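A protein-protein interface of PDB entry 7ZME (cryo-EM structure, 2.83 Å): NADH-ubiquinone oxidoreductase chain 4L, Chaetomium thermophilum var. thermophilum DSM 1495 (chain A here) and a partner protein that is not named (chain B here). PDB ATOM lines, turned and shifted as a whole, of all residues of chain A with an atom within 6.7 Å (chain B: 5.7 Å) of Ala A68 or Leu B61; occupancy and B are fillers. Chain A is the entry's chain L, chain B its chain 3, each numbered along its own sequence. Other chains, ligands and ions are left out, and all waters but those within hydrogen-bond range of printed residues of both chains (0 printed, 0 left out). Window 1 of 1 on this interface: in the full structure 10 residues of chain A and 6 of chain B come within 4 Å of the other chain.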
ATOM      1  N   LEU A  26      -7.906 -13.703  25.432  1.00  0.00           N
ATOM      2  CA  LEU A  26      -8.403 -12.412  24.883  1.00  0.00           C
ATOM      3  C   LEU A  26      -7.564 -11.241  25.424  1.00  0.00           C
ATOM      4  O   LEU A  26      -7.450 -10.237  24.706  1.00  0.00           O
ATOM      5  CB  LEU A  26      -9.873 -12.298  25.301  1.00  0.00           C
ATOM      6  CG  LEU A  26     -10.671 -11.137  24.718  1.00  0.00           C
ATOM      7  CD1 LEU A  26     -10.699 -11.198  23.200  1.00  0.00           C
ATOM      8  CD2 LEU A  26     -12.085 -11.141  25.271  1.00  0.00           C
ATOM      9  N   ALA A  63      -9.389  -2.641  18.433  1.00  0.00           N
ATOM     10  CA  ALA A  63      -8.992  -3.504  19.538  1.00  0.00           C
ATOM     11  C   ALA A  63     -10.109  -3.625  20.563  1.00  0.00           C
ATOM     12  O   ALA A  63     -10.298  -4.690  21.161  1.00  0.00           O
ATOM     13  CB  ALA A  63      -7.719  -2.971  20.191  1.00  0.00           C
ATOM     14  N   GLY A  64     -10.852  -2.539  20.787  1.00  0.00           N
ATOM     15  CA  GLY A  64     -11.985  -2.606  21.691  1.00  0.00           C
ATOM     16  C   GLY A  64     -13.188  -3.278  21.064  1.00  0.00           C
ATOM     17  O   GLY A  64     -13.951  -3.964  21.747  1.00  0.00           O
ATOM     18  N   ALA A  65     -13.376  -3.087  19.758  1.00  0.00           N
ATOM     19  CA  ALA A  65     -14.446  -3.784  19.054  1.00  0.00           C
ATOM     20  C   ALA A  65     -14.214  -5.288  19.062  1.00  0.00           C
ATOM     21  O   ALA A  65     -15.161  -6.071  19.198  1.00  0.00           O
ATOM     22  CB  ALA A  65     -14.561  -3.261  17.623  1.00  0.00           C
ATOM     23  N   GLU A  66     -12.959  -5.711  18.911  1.00  0.00           N
ATOM     24  CA  GLU A  66     -12.640  -7.132  18.976  1.00  0.00           C
ATOM     25  C   GLU A  66     -12.870  -7.687  20.375  1.00  0.00           C
ATOM     26  O   GLU A  66     -13.318  -8.829  20.530  1.00  0.00           O
ATOM     27  CB  GLU A  66     -11.195  -7.360  18.531  1.00  0.00           C
ATOM     28  CG  GLU A  66     -10.647  -8.735  18.858  1.00  0.00           C
ATOM     29  CD  GLU A  66      -9.248  -8.944  18.323  1.00  0.00           C
ATOM     30  OE1 GLU A  66      -8.639  -7.960  17.857  1.00  0.00           O
ATOM     31  OE2 GLU A  66      -8.759 -10.092  18.366  1.00  0.00           O
ATOM     32  N   SER A  67     -12.578  -6.895  21.407  1.00  0.00           N
ATOM     33  CA  SER A  67     -12.772  -7.368  22.772  1.00  0.00           C
ATOM     34  C   SER A  67     -14.247  -7.430  23.145  1.00  0.00           C
ATOM     35  O   SER A  67     -14.626  -8.202  24.030  1.00  0.00           O
ATOM     36  CB  SER A  67     -12.001  -6.480  23.749  1.00  0.00           C
ATOM     37  OG  SER A  67     -12.542  -5.174  23.797  1.00  0.00           O
ATOM     38  N   ALA A  68     -15.091  -6.635  22.487  1.00  0.00           N
ATOM     39  CA  ALA A  68     -16.529  -6.741  22.700  1.00  0.00           C
ATOM     40  C   ALA A  68     -17.103  -7.985  22.034  1.00  0.00           C
ATOM     41  O   ALA A  68     -17.944  -8.674  22.620  1.00  0.00           O
ATOM     42  CB  ALA A  68     -17.233  -5.488  22.184  1.00  0.00           C
ATOM     43  N   ILE A  69     -16.669  -8.282  20.808  1.00  0.00           N
ATOM     44  CA  ILE A  69     -17.118  -9.494  20.133  1.00  0.00           C
ATOM     45  C   ILE A  69     -16.582 -10.729  20.842  1.00  0.00           C
ATOM     46  O   ILE A  69     -17.267 -11.753  20.936  1.00  0.00           O
ATOM     47  CB  ILE A  69     -16.707  -9.460  18.648  1.00  0.00           C
ATOM     48  CG1 ILE A  69     -17.267  -8.212  17.979  1.00  0.00           C
ATOM     49  CG2 ILE A  69     -17.184 -10.705  17.919  1.00  0.00           C
ATOM     50  CD1 ILE A  69     -18.766  -8.171  17.966  1.00  0.00           C
ATOM     51  N   GLY A  70     -15.356 -10.653  21.359  1.00  0.00           N
ATOM     52  CA  GLY A  70     -14.814 -11.770  22.111  1.00  0.00           C
ATOM     53  C   GLY A  70     -15.548 -12.019  23.413  1.00  0.00           C
ATOM     54  O   GLY A  70     -15.839 -13.166  23.759  1.00  0.00           O
ATOM     55  N   LEU A  71     -15.849 -10.955  24.157  1.00  0.00           N
ATOM     56  CA  LEU A  71     -16.586 -11.123  25.402  1.00  0.00           C
ATOM     57  C   LEU A  71     -18.015 -11.569  25.133  1.00  0.00           C
ATOM     58  O   LEU A  71     -18.582 -12.351  25.902  1.00  0.00           O
ATOM     59  CB  LEU A  71     -16.563  -9.824  26.209  1.00  0.00           C
ATOM     60  CG  LEU A  71     -15.282  -9.566  27.005  1.00  0.00           C
ATOM     61  CD1 LEU A  71     -15.397  -8.300  27.816  1.00  0.00           C
ATOM     62  CD2 LEU A  71     -14.952 -10.748  27.897  1.00  0.00           C
ATOM     63  N   GLY A  72     -18.611 -11.082  24.044  1.00  0.00           N
ATOM     64  CA  GLY A  72     -19.947 -11.521  23.682  1.00  0.00           C
ATOM     65  C   GLY A  72     -19.996 -12.976  23.261  1.00  0.00           C
ATOM     66  O   GLY A  72     -20.960 -13.684  23.563  1.00  0.00           O
ATOM     67  N   ILE A  73     -18.967 -13.441  22.552  1.00  0.00           N
ATOM     68  CA  ILE A  73     -18.932 -14.838  22.137  1.00  0.00           C
ATOM     69  C   ILE A  73     -18.618 -15.740  23.323  1.00  0.00           C
ATOM     70  O   ILE A  73     -19.120 -16.867  23.404  1.00  0.00           O
ATOM     71  CB  ILE A  73     -17.936 -15.029  20.974  1.00  0.00           C
ATOM     72  CG1 ILE A  73     -18.523 -14.452  19.686  1.00  0.00           C
ATOM     73  CG2 ILE A  73     -17.610 -16.496  20.765  1.00  0.00           C
ATOM     74  CD1 ILE A  73     -17.542 -14.342  18.554  1.00  0.00           C
ATOM     75  N   VAL A  75     -19.680 -15.211  26.392  1.00  0.00           N
ATOM     76  CA  VAL A  75     -20.930 -15.354  27.130  1.00  0.00           C
ATOM     77  C   VAL A  75     -21.800 -16.422  26.480  1.00  0.00           C
ATOM     78  O   VAL A  75     -22.332 -17.308  27.155  1.00  0.00           O
ATOM     79  CB  VAL A  75     -21.655 -14.001  27.222  1.00  0.00           C
ATOM     80  CG1 VAL A  75     -23.099 -14.195  27.635  1.00  0.00           C
ATOM     81  CG2 VAL A  75     -20.948 -13.106  28.201  1.00  0.00           C
ATOM     82  N   PHE B  57     -24.512  -6.970  31.915  1.00  0.00           N
ATOM     83  CA  PHE B  57     -23.242  -7.170  31.167  1.00  0.00           C
ATOM     84  C   PHE B  57     -23.389  -6.638  29.733  1.00  0.00           C
ATOM     85  O   PHE B  57     -22.375  -6.276  29.120  1.00  0.00           O
ATOM     86  CB  PHE B  57     -22.821  -8.639  31.239  1.00  0.00           C
ATOM     87  CG  PHE B  57     -23.576  -9.551  30.309  1.00  0.00           C
ATOM     88  CD1 PHE B  57     -23.116  -9.784  29.024  1.00  0.00           C
ATOM     89  CD2 PHE B  57     -24.750 -10.164  30.714  1.00  0.00           C
ATOM     90  CE1 PHE B  57     -23.819 -10.607  28.161  1.00  0.00           C
ATOM     91  CE2 PHE B  57     -25.445 -10.994  29.852  1.00  0.00           C
ATOM     92  CZ  PHE B  57     -24.977 -11.213  28.580  1.00  0.00           C
ATOM     93  N   ILE B  58     -24.614  -6.611  29.218  1.00  0.00           N
ATOM     94  CA  ILE B  58     -24.892  -6.101  27.845  1.00  0.00           C
ATOM     95  C   ILE B  58     -24.654  -4.585  27.849  1.00  0.00           C
ATOM     96  O   ILE B  58     -24.290  -4.043  26.797  1.00  0.00           O
ATOM     97  CB  ILE B  58     -26.300  -6.545  27.390  1.00  0.00           C
ATOM     98  CG1 ILE B  58     -26.432  -8.069  27.389  1.00  0.00           C
ATOM     99  CG2 ILE B  58     -26.674  -5.953  26.045  1.00  0.00           C
ATOM    100  CD1 ILE B  58     -27.779  -8.570  26.935  1.00  0.00           C
ATOM    101  N   TYR B  59     -24.741  -3.955  29.023  1.00  0.00           N
ATOM    102  CA  TYR B  59     -24.490  -2.499  29.158  1.00  0.00           C
ATOM    103  C   TYR B  59     -22.975  -2.281  29.166  1.00  0.00           C
ATOM    104  O   TYR B  59     -22.529  -1.264  28.633  1.00  0.00           O
ATOM    105  CB  TYR B  59     -24.982  -1.993  30.516  1.00  0.00           C
ATOM    106  CG  TYR B  59     -26.428  -1.601  30.667  1.00  0.00           C
ATOM    107  CD1 TYR B  59     -27.401  -2.534  30.978  1.00  0.00           C
ATOM    108  CD2 TYR B  59     -26.808  -0.276  30.585  1.00  0.00           C
ATOM    109  CE1 TYR B  59     -28.724  -2.165  31.153  1.00  0.00           C
ATOM    110  CE2 TYR B  59     -28.125   0.110  30.757  1.00  0.00           C
ATOM    111  CZ  TYR B  59     -29.087  -0.836  31.043  1.00  0.00           C
ATOM    112  OH  TYR B  59     -30.384  -0.446  31.208  1.00  0.00           O
ATOM    113  N   GLY B  60     -22.213  -3.193  29.774  1.00  0.00           N
ATOM    114  CA  GLY B  60     -20.768  -3.070  29.689  1.00  0.00           C
ATOM    115  C   GLY B  60     -20.242  -3.277  28.283  1.00  0.00           C
ATOM    116  O   GLY B  60     -19.292  -2.615  27.863  1.00  0.00           O
ATOM    117  N   LEU B  61     -20.818  -4.216  27.538  1.00  0.00           N
ATOM    118  CA  LEU B  61     -20.391  -4.434  26.134  1.00  0.00           C
ATOM    119  C   LEU B  61     -20.617  -3.155  25.321  1.00  0.00           C
ATOM    120  O   LEU B  61     -19.707  -2.784  24.572  1.00  0.00           O
ATOM    121  CB  LEU B  61     -21.166  -5.622  25.562  1.00  0.00           C
ATOM    122  CG  LEU B  61     -20.759  -6.997  26.084  1.00  0.00           C
ATOM    123  CD1 LEU B  61     -21.729  -8.066  25.608  1.00  0.00           C
ATOM    124  CD2 LEU B  61     -19.343  -7.337  25.652  1.00  0.00           C
ATOM    125  N   VAL B  62     -21.792  -2.530  25.439  1.00  0.00           N
ATOM    126  CA  VAL B  62     -22.139  -1.287  24.685  1.00  0.00           C
ATOM    127  C   VAL B  62     -21.286  -0.099  25.142  1.00  0.00           C
ATOM    128  O   VAL B  62     -20.917   0.710  24.285  1.00  0.00           O
ATOM    129  CB  VAL B  62     -23.651  -0.994  24.741  1.00  0.00           C
ATOM    130  CG1 VAL B  62     -24.464  -2.065  24.034  1.00  0.00           C
ATOM    131  CG2 VAL B  62     -24.140  -0.796  26.166  1.00  0.00           C
ATOM    132  N   PHE B  63     -20.992   0.002  26.439  1.00  0.00           N
ATOM    133  CA  PHE B  63     -20.208   1.131  27.002  1.00  0.00           C
ATOM    134  C   PHE B  63     -18.827   1.171  26.358  1.00  0.00           C
ATOM    135  O   PHE B  63     -18.346   2.272  26.091  1.00  0.00           O
ATOM    136  CB  PHE B  63     -20.119   0.977  28.523  1.00  0.00           C
ATOM    137  CG  PHE B  63     -18.843   1.439  29.181  1.00  0.00           C
ATOM    138  CD1 PHE B  63     -18.694   2.747  29.599  1.00  0.00           C
ATOM    139  CD2 PHE B  63     -17.805   0.555  29.422  1.00  0.00           C
ATOM    140  CE1 PHE B  63     -17.523   3.177  30.197  1.00  0.00           C
ATOM    141  CE2 PHE B  63     -16.633   0.986  30.019  1.00  0.00           C
ATOM    142  CZ  PHE B  63     -16.494   2.295  30.409  1.00  0.00           C
ATOM    143  N   LEU B  64     -18.227   0.006  26.123  1.00  0.00           N
ATOM    144  CA  LEU B  64     -16.867  -0.057  25.542  1.00  0.00           C
ATOM    145  C   LEU B  64     -16.870   0.579  24.156  1.00  0.00           C
ATOM    146  O   LEU B  64     -15.995   1.414  23.899  1.00  0.00           O
ATOM    147  CB  LEU B  64     -16.494  -1.537  25.413  1.00  0.00           C
ATOM    148  CG  LEU B  64     -16.243  -2.284  26.718  1.00  0.00           C
ATOM    149  CD1 LEU B  64     -15.774  -3.700  26.435  1.00  0.00           C
ATOM    150  CD2 LEU B  64     -15.225  -1.544  27.562  1.00  0.00           C
ATOM    151  N   LEU B  65     -17.840   0.221  23.324  1.00  0.00           N
ATOM    152  CA  LEU B  65     -17.917   0.743  21.942  1.00  0.00           C
ATOM    153  C   LEU B  65     -18.231   2.240  21.926  1.00  0.00           C
ATOM    154  O   LEU B  65     -17.602   2.954  21.145  1.00  0.00           O
ATOM    155  CB  LEU B  65     -18.980  -0.070  21.200  1.00  0.00           C
ATOM    156  CG  LEU B  65     -18.811  -1.585  21.297  1.00  0.00           C
ATOM    157  CD1 LEU B  65     -20.072  -2.305  20.854  1.00  0.00           C
ATOM    158  CD2 LEU B  65     -17.607  -2.050  20.494  1.00  0.00           C
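Gly A64 touches none of the printed residues of chain B.
Of the printed residues of chain B, Ala A65 touches Leu B65.
Ala A68 touches just these residues of chain B: Leu B61 (3.6 Å) and Leu B65 (3.8 Å).
Printed residues of chain B within 4 Å of Leu A71: Leu B61 (3.8 Å).
Printed residues of chain A within 4 Å of Phe B57: Val A75.
Leu B61 touches two residues of chain A.
Of the printed residues of chain A, Leu B65 touches Ala A65 and Ala A68.
The nearest residue of chain A that does not touch Leu B61 is Gly A72 (4.1 Å).
The nearest printed residue of chain B that does not touch Leu A71 is Leu B64 (4.8 Å).
Leu B65 touches Ala A65.
Leu B61 touches Ala A68.
Ala A68 touches Leu B65.
Leu A71 touches Leu B61.
Val A75 touches Phe B57.
Hydrophobic or aromatic side chains of chain A within 4 Å of the printed part of chain B: Ala A68, Leu A71 and Val A75.
Printed residues of chain B that touch a printed residue of chain A: Phe B57, Leu B61 and Leu B65.
Along chain B the printed residues that touch a printed residue of chain A span positions 57 to 65.
Among the printed residues, no Asp or Glu carboxylate lies within 4 Å of a Lys or Arg side-chain nitrogen of the other chain.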
